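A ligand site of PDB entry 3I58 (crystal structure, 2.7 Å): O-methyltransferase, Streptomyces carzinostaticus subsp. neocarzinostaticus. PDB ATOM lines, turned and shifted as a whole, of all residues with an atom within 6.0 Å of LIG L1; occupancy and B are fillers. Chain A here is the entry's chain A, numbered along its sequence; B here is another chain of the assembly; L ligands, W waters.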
ATOM      1  N   TRP A  96      -6.911  15.870 -18.385  1.00  0.00           N
ATOM      2  CA  TRP A  96      -6.360  16.916 -19.250  1.00  0.00           C
ATOM      3  C   TRP A  96      -5.577  17.964 -18.459  1.00  0.00           C
ATOM      4  O   TRP A  96      -4.693  18.636 -18.996  1.00  0.00           O
ATOM      5  CB  TRP A  96      -7.463  17.616 -20.031  1.00  0.00           C
ATOM      6  CG  TRP A  96      -8.023  16.804 -21.157  1.00  0.00           C
ATOM      7  CD1 TRP A  96      -9.019  15.881 -21.080  1.00  0.00           C
ATOM      8  CD2 TRP A  96      -7.597  16.827 -22.533  1.00  0.00           C
ATOM      9  NE1 TRP A  96      -9.248  15.326 -22.318  1.00  0.00           N
ATOM     10  CE2 TRP A  96      -8.385  15.886 -23.228  1.00  0.00           C
ATOM     11  CE3 TRP A  96      -6.617  17.546 -23.230  1.00  0.00           C
ATOM     12  CZ2 TRP A  96      -8.237  15.648 -24.601  1.00  0.00           C
ATOM     13  CZ3 TRP A  96      -6.468  17.308 -24.603  1.00  0.00           C
ATOM     14  CH2 TRP A  96      -7.270  16.362 -25.264  1.00  0.00           C
ATOM     15  N   VAL A 103      -0.623  16.652 -22.113  1.00  0.00           N
ATOM     16  CA  VAL A 103      -1.262  17.951 -22.261  1.00  0.00           C
ATOM     17  C   VAL A 103      -1.176  18.817 -20.990  1.00  0.00           C
ATOM     18  O   VAL A 103      -1.027  20.025 -21.070  1.00  0.00           O
ATOM     19  CB  VAL A 103      -2.738  17.793 -22.701  1.00  0.00           C
ATOM     20  CG1 VAL A 103      -3.456  19.130 -22.663  1.00  0.00           C
ATOM     21  CG2 VAL A 103      -2.785  17.222 -24.103  1.00  0.00           C
ATOM     22  N   ASP A 107       0.891  22.293 -21.503  1.00  0.00           N
ATOM     23  CA  ASP A 107       0.198  23.556 -21.237  1.00  0.00           C
ATOM     24  C   ASP A 107       1.027  24.473 -20.340  1.00  0.00           C
ATOM     25  O   ASP A 107       0.928  25.694 -20.457  1.00  0.00           O
ATOM     26  CB  ASP A 107      -1.173  23.303 -20.616  1.00  0.00           C
ATOM     27  CG  ASP A 107      -2.286  23.290 -21.642  1.00  0.00           C
ATOM     28  OD1 ASP A 107      -1.986  23.071 -22.840  1.00  0.00           O
ATOM     29  OD2 ASP A 107      -3.454  23.493 -21.269  1.00  0.00           O
ATOM     30  N   PHE A 132       8.296  18.555 -28.396  1.00  0.00           N
ATOM     31  CA  PHE A 132       7.226  17.778 -27.797  1.00  0.00           C
ATOM     32  C   PHE A 132       7.365  16.317 -28.203  1.00  0.00           C
ATOM     33  O   PHE A 132       7.318  15.426 -27.357  1.00  0.00           O
ATOM     34  CB  PHE A 132       5.893  18.349 -28.273  1.00  0.00           C
ATOM     35  CG  PHE A 132       4.686  17.731 -27.620  1.00  0.00           C
ATOM     36  CD1 PHE A 132       4.390  17.995 -26.289  1.00  0.00           C
ATOM     37  CD2 PHE A 132       3.808  16.938 -28.358  1.00  0.00           C
ATOM     38  CE1 PHE A 132       3.221  17.487 -25.703  1.00  0.00           C
ATOM     39  CE2 PHE A 132       2.648  16.429 -27.783  1.00  0.00           C
ATOM     40  CZ  PHE A 132       2.358  16.716 -26.449  1.00  0.00           C
ATOM     41  N   PHE A 146      -0.557  10.772 -23.856  1.00  0.00           N
ATOM     42  CA  PHE A 146      -0.958  11.567 -25.009  1.00  0.00           C
ATOM     43  C   PHE A 146      -1.916  10.739 -25.884  1.00  0.00           C
ATOM     44  O   PHE A 146      -2.940  11.248 -26.327  1.00  0.00           O
ATOM     45  CB  PHE A 146       0.264  12.034 -25.809  1.00  0.00           C
ATOM     46  CG  PHE A 146      -0.064  13.064 -26.859  1.00  0.00           C
ATOM     47  CD1 PHE A 146      -0.667  14.267 -26.503  1.00  0.00           C
ATOM     48  CD2 PHE A 146       0.147  12.797 -28.200  1.00  0.00           C
ATOM     49  CE1 PHE A 146      -1.060  15.187 -27.462  1.00  0.00           C
ATOM     50  CE2 PHE A 146      -0.237  13.717 -29.170  1.00  0.00           C
ATOM     51  CZ  PHE A 146      -0.848  14.920 -28.803  1.00  0.00           C
ATOM     52  N   MET A 150      -5.731  11.971 -27.009  1.00  0.00           N
ATOM     53  CA  MET A 150      -6.221  12.170 -28.369  1.00  0.00           C
ATOM     54  C   MET A 150      -7.362  11.211 -28.620  1.00  0.00           C
ATOM     55  O   MET A 150      -8.281  11.496 -29.378  1.00  0.00           O
ATOM     56  CB  MET A 150      -5.109  11.937 -29.386  1.00  0.00           C
ATOM     57  CG  MET A 150      -3.956  12.941 -29.306  1.00  0.00           C
ATOM     58  SD  MET A 150      -4.520  14.622 -29.572  1.00  0.00           S
ATOM     59  CE  MET A 150      -4.611  15.157 -27.882  1.00  0.00           C
ATOM     60  N   HIS A 153     -10.284  12.934 -27.291  1.00  0.00           N
ATOM     61  CA  HIS A 153     -10.649  14.058 -28.144  1.00  0.00           C
ATOM     62  C   HIS A 153     -11.564  13.586 -29.293  1.00  0.00           C
ATOM     63  O   HIS A 153     -12.426  14.342 -29.763  1.00  0.00           O
ATOM     64  CB  HIS A 153      -9.371  14.750 -28.659  1.00  0.00           C
ATOM     65  CG  HIS A 153      -9.197  14.733 -30.150  1.00  0.00           C
ATOM     66  ND1 HIS A 153      -9.829  15.614 -30.986  1.00  0.00           N
ATOM     67  CD2 HIS A 153      -8.429  13.949 -30.949  1.00  0.00           C
ATOM     68  CE1 HIS A 153      -9.473  15.374 -32.237  1.00  0.00           C
ATOM     69  NE2 HIS A 153      -8.620  14.368 -32.239  1.00  0.00           N
ATOM     70  N   ASP A 157     -14.965  15.425 -30.117  1.00  0.00           N
ATOM     71  CA  ASP A 157     -15.194  16.181 -31.341  1.00  0.00           C
ATOM     72  C   ASP A 157     -15.726  15.484 -32.587  1.00  0.00           C
ATOM     73  O   ASP A 157     -16.405  16.102 -33.405  1.00  0.00           O
ATOM     74  CB  ASP A 157     -13.908  16.925 -31.747  1.00  0.00           C
ATOM     75  CG  ASP A 157     -13.194  17.588 -30.566  1.00  0.00           C
ATOM     76  OD1 ASP A 157     -13.866  18.259 -29.767  1.00  0.00           O
ATOM     77  OD2 ASP A 157     -11.951  17.444 -30.451  1.00  0.00           O
ATOM     78  N   ALA A 243      -6.277  15.800 -37.162  1.00  0.00           N
ATOM     79  CA  ALA A 243      -5.656  16.637 -36.124  1.00  0.00           C
ATOM     80  C   ALA A 243      -4.141  16.527 -36.187  1.00  0.00           C
ATOM     81  O   ALA A 243      -3.473  16.385 -35.158  1.00  0.00           O
ATOM     82  CB  ALA A 243      -6.176  16.230 -34.743  1.00  0.00           C
ATOM     83  N   HIS A 246      -2.487  20.915 -37.958  1.00  0.00           N
ATOM     84  CA  HIS A 246      -2.344  22.044 -37.051  1.00  0.00           C
ATOM     85  C   HIS A 246      -1.159  21.913 -36.076  1.00  0.00           C
ATOM     86  O   HIS A 246      -0.833  22.847 -35.365  1.00  0.00           O
ATOM     87  CB  HIS A 246      -3.667  22.299 -36.319  1.00  0.00           C
ATOM     88  CG  HIS A 246      -4.059  21.225 -35.349  1.00  0.00           C
ATOM     89  ND1 HIS A 246      -5.368  20.994 -34.993  1.00  0.00           N
ATOM     90  CD2 HIS A 246      -3.314  20.370 -34.607  1.00  0.00           C
ATOM     91  CE1 HIS A 246      -5.424  20.057 -34.070  1.00  0.00           C
ATOM     92  NE2 HIS A 246      -4.186  19.662 -33.810  1.00  0.00           N
ATOM     93  N   ASP A 247      -0.510  20.753 -36.062  1.00  0.00           N
ATOM     94  CA  ASP A 247       0.640  20.555 -35.189  1.00  0.00           C
ATOM     95  C   ASP A 247       1.920  21.032 -35.884  1.00  0.00           C
ATOM     96  O   ASP A 247       2.975  21.035 -35.256  1.00  0.00           O
ATOM     97  CB  ASP A 247       0.842  19.079 -34.845  1.00  0.00           C
ATOM     98  CG  ASP A 247      -0.293  18.496 -34.042  1.00  0.00           C
ATOM     99  OD1 ASP A 247      -1.036  19.266 -33.410  1.00  0.00           O
ATOM    100  OD2 ASP A 247      -0.433  17.243 -34.024  1.00  0.00           O
ATOM    101  N   MET A 286      -6.913  27.713 -28.740  1.00  0.00           N
ATOM    102  CA  MET A 286      -6.300  26.522 -29.311  1.00  0.00           C
ATOM    103  C   MET A 286      -5.182  26.913 -30.266  1.00  0.00           C
ATOM    104  O   MET A 286      -4.145  26.269 -30.320  1.00  0.00           O
ATOM    105  CB  MET A 286      -7.326  25.675 -30.068  1.00  0.00           C
ATOM    106  CG  MET A 286      -6.762  24.343 -30.561  1.00  0.00           C
ATOM    107  SD  MET A 286      -6.242  23.177 -29.233  1.00  0.00           S
ATOM    108  CE  MET A 286      -7.086  21.687 -29.776  1.00  0.00           C
ATOM    109  N   ARG A 289      -2.091  27.451 -28.398  1.00  0.00           N
ATOM    110  CA  ARG A 289      -1.541  26.221 -27.850  1.00  0.00           C
ATOM    111  C   ARG A 289      -0.683  25.553 -28.944  1.00  0.00           C
ATOM    112  O   ARG A 289       0.424  25.096 -28.672  1.00  0.00           O
ATOM    113  CB  ARG A 289      -2.652  25.281 -27.389  1.00  0.00           C
ATOM    114  CG  ARG A 289      -2.156  23.918 -26.891  1.00  0.00           C
ATOM    115  CD  ARG A 289      -2.929  23.451 -25.662  1.00  0.00           C
ATOM    116  NE  ARG A 289      -4.349  23.692 -25.846  1.00  0.00           N
ATOM    117  CZ  ARG A 289      -5.205  23.867 -24.853  1.00  0.00           C
ATOM    118  NH1 ARG A 289      -4.789  23.836 -23.596  1.00  0.00           N
ATOM    119  NH2 ARG A 289      -6.476  24.112 -25.128  1.00  0.00           N
ATOM    120  N   MET A 290      -1.196  25.524 -30.173  1.00  0.00           N
ATOM    121  CA  MET A 290      -0.441  24.932 -31.286  1.00  0.00           C
ATOM    122  C   MET A 290       0.871  25.682 -31.487  1.00  0.00           C
ATOM    123  O   MET A 290       1.902  25.084 -31.815  1.00  0.00           O
ATOM    124  CB  MET A 290      -1.269  24.979 -32.573  1.00  0.00           C
ATOM    125  CG  MET A 290      -2.498  24.078 -32.548  1.00  0.00           C
ATOM    126  SD  MET A 290      -2.074  22.356 -32.180  1.00  0.00           S
ATOM    127  CE  MET A 290      -2.802  22.161 -30.553  1.00  0.00           C
ATOM    128  N   TYR A 293       3.173  24.850 -28.372  1.00  0.00           N
ATOM    129  CA  TYR A 293       3.580  23.443 -28.375  1.00  0.00           C
ATOM    130  C   TYR A 293       4.541  23.090 -29.507  1.00  0.00           C
ATOM    131  O   TYR A 293       5.632  22.589 -29.263  1.00  0.00           O
ATOM    132  CB  TYR A 293       2.379  22.504 -28.530  1.00  0.00           C
ATOM    133  CG  TYR A 293       1.680  22.107 -27.267  1.00  0.00           C
ATOM    134  CD1 TYR A 293       1.191  23.068 -26.385  1.00  0.00           C
ATOM    135  CD2 TYR A 293       1.431  20.769 -26.972  1.00  0.00           C
ATOM    136  CE1 TYR A 293       0.462  22.704 -25.253  1.00  0.00           C
ATOM    137  CE2 TYR A 293       0.704  20.396 -25.838  1.00  0.00           C
ATOM    138  CZ  TYR A 293       0.216  21.370 -24.990  1.00  0.00           C
ATOM    139  OH  TYR A 293      -0.525  21.039 -23.887  1.00  0.00           O
ATOM    140  N   PHE A 294       4.136  23.328 -30.752  1.00  0.00           N
ATOM    141  CA  PHE A 294       5.020  22.974 -31.854  1.00  0.00           C
ATOM    142  C   PHE A 294       5.215  24.017 -32.917  1.00  0.00           C
ATOM    143  O   PHE A 294       5.857  23.751 -33.932  1.00  0.00           O
ATOM    144  CB  PHE A 294       4.566  21.672 -32.549  1.00  0.00           C
ATOM    145  CG  PHE A 294       3.411  20.963 -31.886  1.00  0.00           C
ATOM    146  CD1 PHE A 294       2.121  21.452 -31.978  1.00  0.00           C
ATOM    147  CD2 PHE A 294       3.627  19.770 -31.195  1.00  0.00           C
ATOM    148  CE1 PHE A 294       1.058  20.778 -31.399  1.00  0.00           C
ATOM    149  CE2 PHE A 294       2.559  19.075 -30.609  1.00  0.00           C
ATOM    150  CZ  PHE A 294       1.275  19.573 -30.715  1.00  0.00           C
ATOM    151  N   ARG B  11     -12.073  23.305 -17.185  1.00  0.00           N
ATOM    152  CA  ARG B  11     -10.880  23.508 -17.990  1.00  0.00           C
ATOM    153  C   ARG B  11     -10.626  24.973 -18.291  1.00  0.00           C
ATOM    154  O   ARG B  11      -9.475  25.406 -18.362  1.00  0.00           O
ATOM    155  CB  ARG B  11     -10.960  22.690 -19.286  1.00  0.00           C
ATOM    156  CG  ARG B  11     -10.892  21.173 -19.050  1.00  0.00           C
ATOM    157  CD  ARG B  11     -10.948  20.395 -20.339  1.00  0.00           C
ATOM    158  NE  ARG B  11      -9.719  20.551 -21.115  1.00  0.00           N
ATOM    159  CZ  ARG B  11      -9.533  20.063 -22.337  1.00  0.00           C
ATOM    160  NH1 ARG B  11     -10.491  19.367 -22.946  1.00  0.00           N
ATOM    161  NH2 ARG B  11      -8.381  20.271 -22.961  1.00  0.00           N
HETATM  162  C1  LIG L   1      -6.778  18.231 -31.632  1.00  0.00           C
HETATM  163  C2  LIG L   1      -1.761  19.021 -28.608  1.00  0.00           C
HETATM  164  O1  LIG L   1      -8.219  19.156 -28.324  1.00  0.00           O
HETATM  165  O2  LIG L   1      -8.518  19.901 -26.272  1.00  0.00           O
HETATM  166  O3  LIG L   1      -6.629  20.812 -24.955  1.00  0.00           O
HETATM  167  C3  LIG L   1      -4.409  20.459 -25.713  1.00  0.00           C
HETATM  168  C4  LIG L   1      -3.527  19.978 -26.684  1.00  0.00           C
HETATM  169  C5  LIG L   1      -3.632  18.364 -29.990  1.00  0.00           C
HETATM  170  C6  LIG L   1      -5.885  18.708 -29.194  1.00  0.00           C
HETATM  171  O4  LIG L   1      -5.482  17.704 -31.320  1.00  0.00           O
HETATM  172  C7  LIG L   1      -7.786  19.597 -27.235  1.00  0.00           C
HETATM  173  C8  LIG L   1      -3.137  18.927 -28.817  1.00  0.00           C
HETATM  174  C9  LIG L   1      -5.000  18.257 -30.174  1.00  0.00           C
HETATM  175  C10 LIG L   1      -5.776  20.340 -25.905  1.00  0.00           C
HETATM  176  C11 LIG L   1      -6.272  19.749 -27.059  1.00  0.00           C
HETATM  177  C12 LIG L   1      -4.023  19.388 -27.839  1.00  0.00           C
HETATM  178  C13 LIG L   1      -5.393  19.278 -28.033  1.00  0.00           C
HETATM  179  N1  LG2 L   2      -5.336  10.988 -35.755  1.00  0.00           N
HETATM  180  C1  LG2 L   2      -4.985  11.244 -34.352  1.00  0.00           C
HETATM  181  C2  LG2 L   2      -3.931  12.356 -34.291  1.00  0.00           C
HETATM  182  C3  LG2 L   2      -3.281  12.406 -32.906  1.00  0.00           C
HETATM  183  S1  LG2 L   2      -2.145  13.815 -32.678  1.00  0.00           S
HETATM  184  C4  LG2 L   2      -6.228  11.662 -33.560  1.00  0.00           C
HETATM  185  O1  LG2 L   2      -6.353  11.201 -32.410  1.00  0.00           O
HETATM  186  O2  LG2 L   2      -7.028  12.443 -34.118  1.00  0.00           O
HETATM  187  C5  LG2 L   2      -0.986  13.676 -34.083  1.00  0.00           C
HETATM  188  C6  LG2 L   2      -0.378  12.292 -34.325  1.00  0.00           C
HETATM  189  O3  LG2 L   2       0.737  12.454 -35.215  1.00  0.00           O
HETATM  190  C7  LG2 L   2       0.181  11.644 -33.045  1.00  0.00           C
HETATM  191  O4  LG2 L   2      -0.209  10.270 -33.005  1.00  0.00           O
HETATM  192  C8  LG2 L   2       1.700  11.743 -33.253  1.00  0.00           C
HETATM  193  O5  LG2 L   2       2.342  10.629 -32.634  1.00  0.00           O
HETATM  194  C9  LG2 L   2       1.734  11.535 -34.767  1.00  0.00           C
HETATM  195  N2  LG2 L   2       3.065  11.891 -35.319  1.00  0.00           N
HETATM  196  C10 LG2 L   2       3.835  12.910 -34.925  1.00  0.00           C
HETATM  197  N3  LG2 L   2       4.903  12.993 -35.703  1.00  0.00           N
HETATM  198  C11 LG2 L   2       4.821  12.018 -36.609  1.00  0.00           C
HETATM  199  C12 LG2 L   2       5.600  11.630 -37.699  1.00  0.00           C
HETATM  200  N4  LG2 L   2       6.702  12.298 -38.009  1.00  0.00           N
HETATM  201  N5  LG2 L   2       5.197  10.593 -38.444  1.00  0.00           N
HETATM  202  C13 LG2 L   2       4.087   9.936 -38.168  1.00  0.00           C
HETATM  203  N6  LG2 L   2       3.315  10.277 -37.149  1.00  0.00           N
HETATM  204  C14 LG2 L   2       3.652  11.316 -36.365  1.00  0.00           C
HETATM  205  O   HOH W   1      -9.133  19.170 -33.986  1.00  0.00           O
HETATM  206  O   HOH W   2      -2.693  17.123 -32.583  1.00  0.00           O
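SD of Met 150 sits close to O4 of LIG L1 (3.7 Å). Residues that only touch LIG L1: Trp 96, Val 103, His 153, Ala 243, Met 286, Met 290, Tyr 293 and Phe 294. Hydrophobic or aromatic side chains that line LIG L1: Trp 96, Val 103, Met 150, His 153, Ala 243, His 246, Met 286, Met 290, Tyr 293 and Phe 294. Within 4 Å of LIG L1: Trp 96, Val 103, Met 150, His 153, Ala 243, His 246, Met 286, Arg 289, Met 290, Tyr 293, Phe 294 and Arg 11 of chain B. The nearest printed residue that does not touch LIG L1 is Phe 146 (4.1 Å).
The side-chain sulfur (SD) of Met 290 lies close to a ring nitrogen (NE2) of His 246 (3.8 Å). OH of Tyr 293 is in hydrogen-bond range of OD1 of Asp 107. OH of Tyr 293 sits at hydrogen-bond distance from O of Val 103. NH1 of Arg 289 is in salt-bridge range of OD2 of Asp 107 (2.7 Å). ND1 of His 153 is in hydrogen-bond range of OD2 of Asp 157 (2.9 Å). The side-chain carboxylate (OD1) of Asp 247 sits close to a ring nitrogen (NE2) of His 246, 3.2 Å away.
The guanidinium group of Arg 11 of chain B lies within salt-bridge range of an oxygen (O2) of LIG L1. An oxygen (O2) of LG2 L2 is in hydrogen-bond range of a ring nitrogen (NE2) of His 153 (3.1 Å). O3 of LIG L1 sits at hydrogen-bond distance from NH2 of Arg 289 (3.3 Å). O4 of LIG L1 is in hydrogen-bond range of NE2 of His 246, at 3.4 Å.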
